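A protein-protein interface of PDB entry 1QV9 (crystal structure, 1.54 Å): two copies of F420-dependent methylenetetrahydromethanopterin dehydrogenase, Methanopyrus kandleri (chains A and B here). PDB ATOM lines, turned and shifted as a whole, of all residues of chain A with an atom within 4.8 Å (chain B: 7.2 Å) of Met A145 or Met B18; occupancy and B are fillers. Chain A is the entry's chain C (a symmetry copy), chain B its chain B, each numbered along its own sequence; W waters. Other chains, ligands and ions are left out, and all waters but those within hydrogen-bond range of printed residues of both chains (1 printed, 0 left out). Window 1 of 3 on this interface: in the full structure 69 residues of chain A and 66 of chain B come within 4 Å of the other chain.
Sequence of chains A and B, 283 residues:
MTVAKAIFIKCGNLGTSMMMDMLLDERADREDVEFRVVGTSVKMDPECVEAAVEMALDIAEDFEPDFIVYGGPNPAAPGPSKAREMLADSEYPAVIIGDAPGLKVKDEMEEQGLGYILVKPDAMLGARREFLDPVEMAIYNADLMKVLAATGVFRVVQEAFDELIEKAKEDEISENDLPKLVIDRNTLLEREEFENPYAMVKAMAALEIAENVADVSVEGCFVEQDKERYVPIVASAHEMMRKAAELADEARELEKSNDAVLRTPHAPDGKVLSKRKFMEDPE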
ATOM      1  N   MET A  18     -23.079  -7.661   6.944  1.00  0.00           N
ATOM      2  CA  MET A  18     -23.620  -8.507   8.009  1.00  0.00           C
ATOM      3  C   MET A  18     -23.058  -8.077   9.360  1.00  0.00           C
ATOM      4  O   MET A  18     -23.765  -8.015  10.364  1.00  0.00           O
ATOM      5  CB  MET A  18     -23.224  -9.985   7.818  1.00  0.00           C
ATOM      6  CG  MET A  18     -23.976 -10.771   6.755  1.00  0.00           C
ATOM      7  SD  MET A  18     -23.663 -12.712   6.930  1.00  0.00           S
ATOM      8  CE  MET A  18     -25.183 -13.162   8.025  1.00  0.00           C
ATOM      9  N   MET A  19     -21.765  -7.778   9.375  1.00  0.00           N
ATOM     10  CA  MET A  19     -21.067  -7.429  10.599  1.00  0.00           C
ATOM     11  C   MET A  19     -20.769  -5.971  10.919  1.00  0.00           C
ATOM     12  O   MET A  19     -20.445  -5.663  12.072  1.00  0.00           O
ATOM     13  CB  MET A  19     -19.699  -8.138  10.595  1.00  0.00           C
ATOM     14  CG  MET A  19     -19.668  -9.597  10.990  1.00  0.00           C
ATOM     15  SD  MET A  19     -19.808  -9.737  12.903  1.00  0.00           S
ATOM     16  CE  MET A  19     -21.479 -10.571  12.870  1.00  0.00           C
ATOM     17  N   MET A  22     -22.029  -4.390  14.225  1.00  0.00           N
ATOM     18  CA  MET A  22     -21.591  -5.139  15.392  1.00  0.00           C
ATOM     19  C   MET A  22     -20.111  -4.947  15.720  1.00  0.00           C
ATOM     20  O   MET A  22     -19.712  -5.018  16.886  1.00  0.00           O
ATOM     21  CB  MET A  22     -21.900  -6.622  15.187  1.00  0.00           C
ATOM     22  CG  MET A  22     -23.379  -6.894  15.064  1.00  0.00           C
ATOM     23  SD  MET A  22     -23.686  -8.732  14.641  1.00  0.00           S
ATOM     24  CE  MET A  22     -25.042  -8.508  13.274  1.00  0.00           C
ATOM     25  N   ASN A 141     -21.203 -18.005   3.774  1.00  0.00           N
ATOM     26  CA  ASN A 141     -21.019 -16.810   4.552  1.00  0.00           C
ATOM     27  C   ASN A 141     -20.183 -17.050   5.804  1.00  0.00           C
ATOM     28  O   ASN A 141     -19.515 -16.123   6.268  1.00  0.00           O
ATOM     29  CB  ASN A 141     -22.392 -16.206   4.908  1.00  0.00           C
ATOM     30  CG  ASN A 141     -22.906 -15.319   3.796  1.00  0.00           C
ATOM     31  OD1 ASN A 141     -23.778 -15.712   3.001  1.00  0.00           O
ATOM     32  ND2 ASN A 141     -22.329 -14.126   3.697  1.00  0.00           N
ATOM     33  N   ALA A 142     -20.215 -18.258   6.353  1.00  0.00           N
ATOM     34  CA  ALA A 142     -19.423 -18.530   7.547  1.00  0.00           C
ATOM     35  C   ALA A 142     -17.961 -18.511   7.132  1.00  0.00           C
ATOM     36  O   ALA A 142     -17.130 -17.926   7.843  1.00  0.00           O
ATOM     37  CB  ALA A 142     -19.801 -19.847   8.150  1.00  0.00           C
ATOM     38  N   ASP A 143     -17.653 -19.123   5.990  1.00  0.00           N
ATOM     39  CA  ASP A 143     -16.258 -19.102   5.512  1.00  0.00           C
ATOM     40  C   ASP A 143     -15.792 -17.696   5.174  1.00  0.00           C
ATOM     41  O   ASP A 143     -14.673 -17.287   5.517  1.00  0.00           O
ATOM     42  CB  ASP A 143     -16.089 -20.003   4.278  1.00  0.00           C
ATOM     43  CG  ASP A 143     -16.169 -21.486   4.624  1.00  0.00           C
ATOM     44  OD1 ASP A 143     -15.793 -21.877   5.780  1.00  0.00           O
ATOM     45  OD2 ASP A 143     -16.603 -22.294   3.736  1.00  0.00           O
ATOM     46  N   LEU A 144     -16.637 -16.912   4.511  1.00  0.00           N
ATOM     47  CA  LEU A 144     -16.255 -15.552   4.156  1.00  0.00           C
ATOM     48  C   LEU A 144     -16.046 -14.702   5.407  1.00  0.00           C
ATOM     49  O   LEU A 144     -15.123 -13.900   5.470  1.00  0.00           O
ATOM     50  CB  LEU A 144     -17.352 -14.915   3.277  1.00  0.00           C
ATOM     51  CG  LEU A 144     -17.149 -13.444   2.948  1.00  0.00           C
ATOM     52  CD1 LEU A 144     -15.814 -13.255   2.234  1.00  0.00           C
ATOM     53  CD2 LEU A 144     -18.319 -12.948   2.075  1.00  0.00           C
ATOM     54  N   MET A 145     -16.886 -14.901   6.423  1.00  0.00           N
ATOM     55  CA  MET A 145     -16.782 -14.122   7.654  1.00  0.00           C
ATOM     56  C   MET A 145     -15.438 -14.426   8.331  1.00  0.00           C
ATOM     57  O   MET A 145     -14.749 -13.520   8.836  1.00  0.00           O
ATOM     58  CB  MET A 145     -17.944 -14.479   8.606  1.00  0.00           C
ATOM     59  CG  MET A 145     -17.861 -13.718   9.914  1.00  0.00           C
ATOM     60  SD  MET A 145     -19.505 -14.000  10.983  1.00  0.00           S
ATOM     61  CE  MET A 145     -20.800 -13.231   9.726  1.00  0.00           C
ATOM     62  N   LYS A 146     -15.075 -15.714   8.302  1.00  0.00           N
ATOM     63  CA  LYS A 146     -13.818 -16.129   8.913  1.00  0.00           C
ATOM     64  C   LYS A 146     -12.662 -15.480   8.174  1.00  0.00           C
ATOM     65  O   LYS A 146     -11.719 -14.979   8.801  1.00  0.00           O
ATOM     66  CB  LYS A 146     -13.688 -17.667   8.898  1.00  0.00           C
ATOM     67  CG  LYS A 146     -12.283 -18.176   9.354  1.00  0.00           C
ATOM     68  CD  LYS A 146     -11.951 -17.728  10.718  1.00  0.00           C
ATOM     69  CE  LYS A 146     -10.777 -18.519  11.281  1.00  0.00           C
ATOM     70  NZ  LYS A 146     -11.147 -19.942  11.452  1.00  0.00           N
ATOM     71  N   VAL A 147     -12.737 -15.449   6.846  1.00  0.00           N
ATOM     72  CA  VAL A 147     -11.683 -14.815   6.064  1.00  0.00           C
ATOM     73  C   VAL A 147     -11.597 -13.315   6.406  1.00  0.00           C
ATOM     74  O   VAL A 147     -10.535 -12.810   6.727  1.00  0.00           O
ATOM     75  CB  VAL A 147     -11.934 -14.935   4.544  1.00  0.00           C
ATOM     76  CG1 VAL A 147     -10.961 -14.040   3.782  1.00  0.00           C
ATOM     77  CG2 VAL A 147     -11.794 -16.413   4.108  1.00  0.00           C
ATOM     78  N   LEU A 148     -12.718 -12.592   6.331  1.00  0.00           N
ATOM     79  CA  LEU A 148     -12.654 -11.148   6.594  1.00  0.00           C
ATOM     80  C   LEU A 148     -12.236 -10.800   8.028  1.00  0.00           C
ATOM     81  O   LEU A 148     -11.585  -9.746   8.294  1.00  0.00           O
ATOM     82  CB  LEU A 148     -14.022 -10.515   6.224  1.00  0.00           C
ATOM     83  CG  LEU A 148     -14.455 -10.753   4.769  1.00  0.00           C
ATOM     84  CD1 LEU A 148     -15.873 -10.146   4.589  1.00  0.00           C
ATOM     85  CD2 LEU A 148     -13.523 -10.130   3.783  1.00  0.00           C
ATOM     86  N   ALA A 149     -12.548 -11.688   8.966  1.00  0.00           N
ATOM     87  CA  ALA A 149     -12.179 -11.450  10.370  1.00  0.00           C
ATOM     88  C   ALA A 149     -10.718 -11.781  10.638  1.00  0.00           C
ATOM     89  O   ALA A 149      -9.947 -10.905  11.045  1.00  0.00           O
ATOM     90  CB  ALA A 149     -13.052 -12.264  11.315  1.00  0.00           C
ATOM     91  N   ALA A 150     -10.342 -13.032  10.376  1.00  0.00           N
ATOM     92  CA  ALA A 150      -8.972 -13.451  10.688  1.00  0.00           C
ATOM     93  C   ALA A 150      -7.869 -12.832   9.863  1.00  0.00           C
ATOM     94  O   ALA A 150      -6.717 -12.875  10.299  1.00  0.00           O
ATOM     95  CB  ALA A 150      -8.858 -14.970  10.679  1.00  0.00           C
ATOM     96  N   PHE A 154     -11.856  -6.836   8.822  1.00  0.00           N
ATOM     97  CA  PHE A 154     -12.853  -6.227   9.705  1.00  0.00           C
ATOM     98  C   PHE A 154     -12.252  -5.189  10.641  1.00  0.00           C
ATOM     99  O   PHE A 154     -12.963  -4.280  11.075  1.00  0.00           O
ATOM    100  CB  PHE A 154     -13.588  -7.288  10.515  1.00  0.00           C
ATOM    101  CG  PHE A 154     -14.633  -8.033   9.734  1.00  0.00           C
ATOM    102  CD1 PHE A 154     -15.108  -9.250  10.204  1.00  0.00           C
ATOM    103  CD2 PHE A 154     -15.182  -7.502   8.562  1.00  0.00           C
ATOM    104  CE1 PHE A 154     -16.129  -9.953   9.525  1.00  0.00           C
ATOM    105  CE2 PHE A 154     -16.202  -8.196   7.878  1.00  0.00           C
ATOM    106  CZ  PHE A 154     -16.667  -9.417   8.364  1.00  0.00           C
ATOM    107  N   LYS B  10     -34.295  -7.437  15.390  1.00  0.00           N
ATOM    108  CA  LYS B  10     -33.027  -7.971  15.905  1.00  0.00           C
ATOM    109  C   LYS B  10     -32.377  -7.079  16.941  1.00  0.00           C
ATOM    110  O   LYS B  10     -31.976  -5.954  16.647  1.00  0.00           O
ATOM    111  CB  LYS B  10     -32.045  -8.184  14.741  1.00  0.00           C
ATOM    112  CG  LYS B  10     -32.557  -9.140  13.701  1.00  0.00           C
ATOM    113  CD  LYS B  10     -31.650  -9.237  12.471  1.00  0.00           C
ATOM    114  CE  LYS B  10     -32.217 -10.251  11.492  1.00  0.00           C
ATOM    115  NZ  LYS B  10     -31.248 -10.645  10.402  1.00  0.00           N
ATOM    116  N   GLY B  12     -29.374  -7.409  19.989  1.00  0.00           N
ATOM    117  CA  GLY B  12     -28.357  -8.287  20.541  1.00  0.00           C
ATOM    118  C   GLY B  12     -28.070  -9.225  19.381  1.00  0.00           C
ATOM    119  O   GLY B  12     -28.624  -9.065  18.297  1.00  0.00           O
ATOM    120  N   ASN B  13     -27.215 -10.212  19.579  1.00  0.00           N
ATOM    121  CA  ASN B  13     -26.941 -11.108  18.467  1.00  0.00           C
ATOM    122  C   ASN B  13     -26.912 -12.582  18.839  1.00  0.00           C
ATOM    123  O   ASN B  13     -26.368 -12.982  19.873  1.00  0.00           O
ATOM    124  CB  ASN B  13     -25.628 -10.715  17.798  1.00  0.00           C
ATOM    125  CG  ASN B  13     -25.382 -11.481  16.514  1.00  0.00           C
ATOM    126  OD1 ASN B  13     -26.201 -11.456  15.583  1.00  0.00           O
ATOM    127  ND2 ASN B  13     -24.248 -12.174  16.457  1.00  0.00           N
ATOM    128  N   LEU B  14     -27.492 -13.372  17.954  1.00  0.00           N
ATOM    129  CA  LEU B  14     -27.577 -14.813  18.079  1.00  0.00           C
ATOM    130  C   LEU B  14     -27.220 -15.316  16.679  1.00  0.00           C
ATOM    131  O   LEU B  14     -27.518 -14.654  15.686  1.00  0.00           O
ATOM    132  CB  LEU B  14     -29.024 -15.172  18.427  1.00  0.00           C
ATOM    133  CG  LEU B  14     -29.399 -16.215  19.463  1.00  0.00           C
ATOM    134  CD1 LEU B  14     -28.536 -16.092  20.694  1.00  0.00           C
ATOM    135  CD2 LEU B  14     -30.870 -16.042  19.794  1.00  0.00           C
ATOM    136  N   GLY B  15     -26.561 -16.469  16.567  1.00  0.00           N
ATOM    137  CA  GLY B  15     -26.259 -16.932  15.235  1.00  0.00           C
ATOM    138  C   GLY B  15     -27.538 -17.124  14.437  1.00  0.00           C
ATOM    139  O   GLY B  15     -27.596 -16.835  13.240  1.00  0.00           O
ATOM    140  N   THR B  16     -28.583 -17.586  15.114  1.00  0.00           N
ATOM    141  CA  THR B  16     -29.830 -17.833  14.416  1.00  0.00           C
ATOM    142  C   THR B  16     -30.523 -16.550  13.990  1.00  0.00           C
ATOM    143  O   THR B  16     -31.151 -16.499  12.931  1.00  0.00           O
ATOM    144  CB  THR B  16     -30.790 -18.637  15.275  1.00  0.00           C
ATOM    145  OG1 THR B  16     -30.169 -19.870  15.637  1.00  0.00           O
ATOM    146  CG2 THR B  16     -32.049 -18.973  14.471  1.00  0.00           C
ATOM    147  N   SER B  17     -30.417 -15.520  14.814  1.00  0.00           N
ATOM    148  CA  SER B  17     -31.065 -14.258  14.483  1.00  0.00           C
ATOM    149  C   SER B  17     -30.336 -13.563  13.341  1.00  0.00           C
ATOM    150  O   SER B  17     -30.929 -12.800  12.567  1.00  0.00           O
ATOM    151  CB  SER B  17     -31.181 -13.368  15.736  1.00  0.00           C
ATOM    152  OG  SER B  17     -29.945 -12.897  16.235  1.00  0.00           O
ATOM    153  N   MET B  18     -29.031 -13.822  13.241  1.00  0.00           N
ATOM    154  CA  MET B  18     -28.229 -13.243  12.170  1.00  0.00           C
ATOM    155  C   MET B  18     -28.768 -13.697  10.825  1.00  0.00           C
ATOM    156  O   MET B  18     -28.942 -12.903   9.907  1.00  0.00           O
ATOM    157  CB  MET B  18     -26.766 -13.714  12.234  1.00  0.00           C
ATOM    158  CG  MET B  18     -25.920 -13.134  13.334  1.00  0.00           C
ATOM    159  SD  MET B  18     -24.015 -13.343  12.919  1.00  0.00           S
ATOM    160  CE  MET B  18     -23.912 -11.905  11.632  1.00  0.00           C
ATOM    161  N   MET B  19     -29.031 -14.995  10.736  1.00  0.00           N
ATOM    162  CA  MET B  19     -29.465 -15.643   9.504  1.00  0.00           C
ATOM    163  C   MET B  19     -30.948 -15.916   9.257  1.00  0.00           C
ATOM    164  O   MET B  19     -31.332 -16.177   8.123  1.00  0.00           O
ATOM    165  CB  MET B  19     -28.716 -16.983   9.380  1.00  0.00           C
ATOM    166  CG  MET B  19     -27.288 -16.895   8.841  1.00  0.00           C
ATOM    167  SD  MET B  19     -27.414 -16.856   6.942  1.00  0.00           S
ATOM    168  CE  MET B  19     -25.854 -15.853   6.471  1.00  0.00           C
ATOM    169  N   MET B  20     -31.772 -15.859  10.298  1.00  0.00           N
ATOM    170  CA  MET B  20     -33.187 -16.204  10.155  1.00  0.00           C
ATOM    171  C   MET B  20     -33.947 -15.722   8.924  1.00  0.00           C
ATOM    172  O   MET B  20     -34.564 -16.530   8.239  1.00  0.00           O
ATOM    173  CB  MET B  20     -33.972 -15.857  11.429  1.00  0.00           C
ATOM    174  CG  MET B  20     -33.870 -14.436  11.895  1.00  0.00           C
ATOM    175  SD  MET B  20     -34.873 -14.188  13.568  1.00  0.00           S
ATOM    176  CE  MET B  20     -34.416 -12.375  13.842  1.00  0.00           C
ATOM    177  N   ASP B  21     -33.892 -14.436   8.617  1.00  0.00           N
ATOM    178  CA  ASP B  21     -34.641 -13.938   7.462  1.00  0.00           C
ATOM    179  C   ASP B  21     -34.066 -14.359   6.117  1.00  0.00           C
ATOM    180  O   ASP B  21     -34.812 -14.656   5.172  1.00  0.00           O
ATOM    181  CB  ASP B  21     -34.762 -12.407   7.535  1.00  0.00           C
ATOM    182  CG  ASP B  21     -33.412 -11.708   7.648  1.00  0.00           C
ATOM    183  OD1 ASP B  21     -32.727 -11.903   8.680  1.00  0.00           O
ATOM    184  OD2 ASP B  21     -33.035 -10.967   6.711  1.00  0.00           O
ATOM    185  N   MET B  22     -32.738 -14.404   6.013  1.00  0.00           N
ATOM    186  CA  MET B  22     -32.124 -14.782   4.749  1.00  0.00           C
ATOM    187  C   MET B  22     -32.310 -16.246   4.402  1.00  0.00           C
ATOM    188  O   MET B  22     -32.239 -16.617   3.237  1.00  0.00           O
ATOM    189  CB  MET B  22     -30.632 -14.458   4.763  1.00  0.00           C
ATOM    190  CG  MET B  22     -30.361 -12.993   4.976  1.00  0.00           C
ATOM    191  SD  MET B  22     -28.493 -12.599   4.832  1.00  0.00           S
ATOM    192  CE  MET B  22     -28.159 -12.121   6.680  1.00  0.00           C
ATOM    193  N   LEU B  23     -32.514 -17.081   5.414  1.00  0.00           N
ATOM    194  CA  LEU B  23     -32.720 -18.493   5.170  1.00  0.00           C
ATOM    195  C   LEU B  23     -34.030 -18.724   4.415  1.00  0.00           C
ATOM    196  O   LEU B  23     -34.266 -19.793   3.870  1.00  0.00           O
ATOM    197  CB  LEU B  23     -32.780 -19.262   6.485  1.00  0.00           C
ATOM    198  CG  LEU B  23     -31.497 -19.350   7.310  1.00  0.00           C
ATOM    199  CD1 LEU B  23     -31.849 -19.903   8.672  1.00  0.00           C
ATOM    200  CD2 LEU B  23     -30.453 -20.245   6.600  1.00  0.00           C
ATOM    201  N   GLY B  71     -35.827 -11.643  17.465  1.00  0.00           N
ATOM    202  CA  GLY B  71     -34.759 -12.607  17.660  1.00  0.00           C
ATOM    203  C   GLY B  71     -33.573 -11.991  18.359  1.00  0.00           C
ATOM    204  O   GLY B  71     -33.143 -10.882  18.024  1.00  0.00           O
ATOM    205  N   ILE B  97     -37.278 -15.869  18.788  1.00  0.00           N
ATOM    206  CA  ILE B  97     -36.135 -16.755  18.526  1.00  0.00           C
ATOM    207  C   ILE B  97     -35.146 -16.454  19.639  1.00  0.00           C
ATOM    208  O   ILE B  97     -34.822 -15.294  19.893  1.00  0.00           O
ATOM    209  CB  ILE B  97     -35.518 -16.449  17.151  1.00  0.00           C
ATOM    210  CG1 ILE B  97     -36.440 -17.020  16.064  1.00  0.00           C
ATOM    211  CG2 ILE B  97     -34.067 -16.989  17.069  1.00  0.00           C
ATOM    212  CD1 ILE B  97     -35.834 -17.037  14.701  1.00  0.00           C
ATOM    213  N   ASP B 122     -27.020 -22.429  20.139  1.00  0.00           N
ATOM    214  CA  ASP B 122     -26.660 -21.039  19.793  1.00  0.00           C
ATOM    215  C   ASP B 122     -26.124 -20.412  21.067  1.00  0.00           C
ATOM    216  O   ASP B 122     -26.800 -19.643  21.756  1.00  0.00           O
ATOM    217  CB  ASP B 122     -27.921 -20.286  19.316  1.00  0.00           C
ATOM    218  CG  ASP B 122     -27.617 -19.129  18.414  1.00  0.00           C
ATOM    219  OD1 ASP B 122     -26.609 -18.424  18.630  1.00  0.00           O
ATOM    220  OD2 ASP B 122     -28.421 -18.903  17.476  1.00  0.00           O
ATOM    221  N   VAL B 135     -12.888  -8.504  16.036  1.00  0.00           N
ATOM    222  CA  VAL B 135     -12.406  -9.622  15.207  1.00  0.00           C
ATOM    223  C   VAL B 135     -12.730 -10.973  15.870  1.00  0.00           C
ATOM    224  O   VAL B 135     -13.258 -11.880  15.216  1.00  0.00           O
ATOM    225  CB  VAL B 135     -10.888  -9.471  14.973  1.00  0.00           C
ATOM    226  CG1 VAL B 135     -10.264 -10.789  14.460  1.00  0.00           C
ATOM    227  CG2 VAL B 135     -10.671  -8.383  13.934  1.00  0.00           C
ATOM    228  N   MET B 137     -15.055 -11.648  17.995  1.00  0.00           N
ATOM    229  CA  MET B 137     -16.496 -11.875  17.936  1.00  0.00           C
ATOM    230  C   MET B 137     -16.912 -12.410  16.549  1.00  0.00           C
ATOM    231  O   MET B 137     -17.734 -13.321  16.436  1.00  0.00           O
ATOM    232  CB  MET B 137     -17.241 -10.572  18.228  1.00  0.00           C
ATOM    233  CG  MET B 137     -18.742 -10.738  18.155  1.00  0.00           C
ATOM    234  SD  MET B 137     -19.418 -10.034  16.498  1.00  0.00           S
ATOM    235  CE  MET B 137     -19.280  -8.186  17.036  1.00  0.00           C
ATOM    236  N   ALA B 138     -16.360 -11.822  15.494  1.00  0.00           N
ATOM    237  CA  ALA B 138     -16.693 -12.255  14.134  1.00  0.00           C
ATOM    238  C   ALA B 138     -16.198 -13.687  13.913  1.00  0.00           C
ATOM    239  O   ALA B 138     -16.894 -14.478  13.308  1.00  0.00           O
ATOM    240  CB  ALA B 138     -16.061 -11.328  13.110  1.00  0.00           C
ATOM    241  N   ILE B 139     -14.997 -14.011  14.404  1.00  0.00           N
ATOM    242  CA  ILE B 139     -14.480 -15.376  14.241  1.00  0.00           C
ATOM    243  C   ILE B 139     -15.404 -16.391  14.914  1.00  0.00           C
ATOM    244  O   ILE B 139     -15.742 -17.429  14.343  1.00  0.00           O
ATOM    245  CB  ILE B 139     -13.045 -15.459  14.842  1.00  0.00           C
ATOM    246  CG1 ILE B 139     -12.094 -14.583  14.022  1.00  0.00           C
ATOM    247  CG2 ILE B 139     -12.567 -16.932  14.933  1.00  0.00           C
ATOM    248  CD1 ILE B 139     -11.807 -15.104  12.665  1.00  0.00           C
ATOM    249  N   TYR B 140     -15.832 -16.084  16.137  1.00  0.00           N
ATOM    250  CA  TYR B 140     -16.703 -16.983  16.874  1.00  0.00           C
ATOM    251  C   TYR B 140     -18.024 -17.143  16.114  1.00  0.00           C
ATOM    252  O   TYR B 140     -18.541 -18.265  15.952  1.00  0.00           O
ATOM    253  CB  TYR B 140     -16.994 -16.404  18.264  1.00  0.00           C
ATOM    254  CG  TYR B 140     -17.960 -17.261  19.050  1.00  0.00           C
ATOM    255  CD1 TYR B 140     -17.516 -18.263  19.911  1.00  0.00           C
ATOM    256  CD2 TYR B 140     -19.343 -17.043  18.947  1.00  0.00           C
ATOM    257  CE1 TYR B 140     -18.412 -19.025  20.668  1.00  0.00           C
ATOM    258  CE2 TYR B 140     -20.234 -17.793  19.691  1.00  0.00           C
ATOM    259  CZ  TYR B 140     -19.770 -18.776  20.554  1.00  0.00           C
ATOM    260  OH  TYR B 140     -20.649 -19.479  21.343  1.00  0.00           O
ATOM    261  N   ASN B 141     -18.558 -16.029  15.623  1.00  0.00           N
ATOM    262  CA  ASN B 141     -19.803 -16.128  14.884  1.00  0.00           C
ATOM    263  C   ASN B 141     -19.653 -16.931  13.594  1.00  0.00           C
ATOM    264  O   ASN B 141     -20.582 -17.621  13.173  1.00  0.00           O
ATOM    265  CB  ASN B 141     -20.394 -14.724  14.624  1.00  0.00           C
ATOM    266  CG  ASN B 141     -21.201 -14.241  15.815  1.00  0.00           C
ATOM    267  OD1 ASN B 141     -20.738 -13.439  16.629  1.00  0.00           O
ATOM    268  ND2 ASN B 141     -22.399 -14.779  15.944  1.00  0.00           N
ATOM    269  N   ALA B 142     -18.483 -16.857  12.956  1.00  0.00           N
ATOM    270  CA  ALA B 142     -18.265 -17.638  11.742  1.00  0.00           C
ATOM    271  C   ALA B 142     -18.309 -19.125  12.093  1.00  0.00           C
ATOM    272  O   ALA B 142     -18.906 -19.929  11.388  1.00  0.00           O
ATOM    273  CB  ALA B 142     -16.899 -17.262  11.120  1.00  0.00           C
ATOM    274  N   ASP B 143     -17.656 -19.502  13.195  1.00  0.00           N
ATOM    275  CA  ASP B 143     -17.663 -20.906  13.585  1.00  0.00           C
ATOM    276  C   ASP B 143     -19.095 -21.370  13.965  1.00  0.00           C
ATOM    277  O   ASP B 143     -19.516 -22.448  13.594  1.00  0.00           O
ATOM    278  CB  ASP B 143     -16.696 -21.166  14.755  1.00  0.00           C
ATOM    279  CG  ASP B 143     -15.234 -21.182  14.308  1.00  0.00           C
ATOM    280  OD1 ASP B 143     -14.986 -21.562  13.140  1.00  0.00           O
ATOM    281  OD2 ASP B 143     -14.355 -20.826  15.140  1.00  0.00           O
ATOM    282  N   MET B 145     -21.903 -20.083  12.967  1.00  0.00           N
ATOM    283  CA  MET B 145     -22.717 -20.102  11.729  1.00  0.00           C
ATOM    284  C   MET B 145     -22.488 -21.394  10.932  1.00  0.00           C
ATOM    285  O   MET B 145     -23.401 -21.972  10.334  1.00  0.00           O
ATOM    286  CB  MET B 145     -22.405 -18.881  10.865  1.00  0.00           C
ATOM    287  CG  MET B 145     -23.166 -18.818   9.539  1.00  0.00           C
ATOM    288  SD  MET B 145     -22.897 -17.100   8.680  1.00  0.00           S
ATOM    289  CE  MET B 145     -23.786 -16.040  10.010  1.00  0.00           C
ATOM    290  N   PHE B 154     -30.189 -24.945  10.765  1.00  0.00           N
ATOM    291  CA  PHE B 154     -30.834 -23.888  10.006  1.00  0.00           C
ATOM    292  C   PHE B 154     -31.940 -24.438   9.104  1.00  0.00           C
ATOM    293  O   PHE B 154     -32.834 -23.686   8.736  1.00  0.00           O
ATOM    294  CB  PHE B 154     -29.827 -23.099   9.164  1.00  0.00           C
ATOM    295  CG  PHE B 154     -28.985 -22.129   9.958  1.00  0.00           C
ATOM    296  CD1 PHE B 154     -27.808 -21.637   9.410  1.00  0.00           C
ATOM    297  CD2 PHE B 154     -29.405 -21.636  11.201  1.00  0.00           C
ATOM    298  CE1 PHE B 154     -27.065 -20.659  10.084  1.00  0.00           C
ATOM    299  CE2 PHE B 154     -28.670 -20.659  11.890  1.00  0.00           C
ATOM    300  CZ  PHE B 154     -27.488 -20.167  11.316  1.00  0.00           C
HETATM  301  O   HOH W   1     -11.939 -20.421  14.375  1.00  0.00           O
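Water W1 bridges OD2 of Asp B143 (2.6 Å) and NZ of Lys A146 (3.1 Å).
The backbone NH (N) of Ala B142 is in hydrogen-bond range of the side-chain sulfur (SD) of Met A145, 3.6 Å away.
N of Ala A142 sits at hydrogen-bond distance from SD of Met B145, at 3.7 Å.
SD of Met B137 sits close to SD of Met A19, at 3.6 Å.
The side-chain sulfur of Met A145 sits close to the backbone carbonyl oxygen of Ala B138 (3.5 Å).
Among the printed residues, merely in contact across the chains: Met A18 with Met B19 (3.2 Å), Met A18 with Met B22 (3.4 Å), Met A18 with Met B145 (3.8 Å), Met A19 with Met B18 (3.0 Å), Met A22 with Asn B13 (3.7 Å), Met A22 with Met B18 (3.9 Å), Met A22 with Met B137 (3.2 Å), Asn A141 with Met B19 (3.8 Å), Asn A141 with Met B145 (3.9 Å), Ala A142 with Ala B142 (3.4 Å), Met A145 with Met B18 (3.9 Å), Met A145 with Asn B141 (3.8 Å), Lys A146 with Ile B139 (3.3 Å), Lys A146 with Ala B142 (3.7 Å), Ala A149 with Val B135 (3.4 Å), Ala A149 with Ala B138 (3.6 Å), Ala A149 with Ile B139 (3.4 Å), Ala A150 with Ile B139 (3.4 Å) and Phe A154 with Ala B138 (3.7 Å).
Met A18 touches Met B19, and with the chains exchanged Met A19 touches Met B18.
Met A18 touches Met B145, and with the chains exchanged Met A145 touches Met B18.
Asn A141 touches Met B19, but with the chains exchanged Met A19 does not touch Asn B141 (4.6 Å).
Asn A141 touches Met B145, and with the chains exchanged Met A145 touches Asn B141.
8 positions are printed for both chains.
Printed residues of chain B within 4 Å of Met A145: Met B18 (3.9 Å), Ala B138 (3.5 Å), Asn B141 (3.8 Å) and Ala B142 (3.6 Å).
Printed residues of chain B within 4 Å of Ala A142: Ala B142 (3.4 Å) and Met B145 (3.7 Å).
Of the printed residues of chain B, Met A22 touches Asn B13, Met B18 and Met B137.
The nearest printed residue of chain B that does not touch Met A145 is Met B145 (4.1 Å).
Of the 14 printed residues of chain A, 10 touch a printed residue of chain B.
Hydrophobic or aromatic side chains of chain A that line the printed part of chain B: Met A18, Met A19, Met A22, Ala A142, Met A145, Ala A149, Ala A150 and Phe A154.
Along chain A the printed residues that touch a printed residue of chain B span positions 18 to 154.
Hydrophobic or aromatic side chains of chain B within 4 Å of the printed part of chain A: Met B18, Met B19, Met B22, Val B135, Met B137, Ala B138, Ile B139, Ala B142 and Met B145.
Among the printed residues, 23 pairs touch across the chains.
Among the printed residues, no Asp or Glu carboxylate lies within 4 Å of a Lys or Arg side-chain nitrogen of the other chain.
The backbone carbonyl oxygen (O) of Met B18 is in hydrogen-bond range of the side-chain amino group (NZ) of Lys B10.
ND2 of Asn B13 lies close to SD of Met B18 (3.7 Å).
ND2 of Asn B141 is in hydrogen-bond range of SD of Met B18 (3.7 Å).
O of Met B137 sits close to OD1 of Asn B141, 3.0 Å away.
The backbone carbonyl oxygen of Leu A148 is in hydrogen-bond range of the backbone NH of Phe A154, at 3.0 Å.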
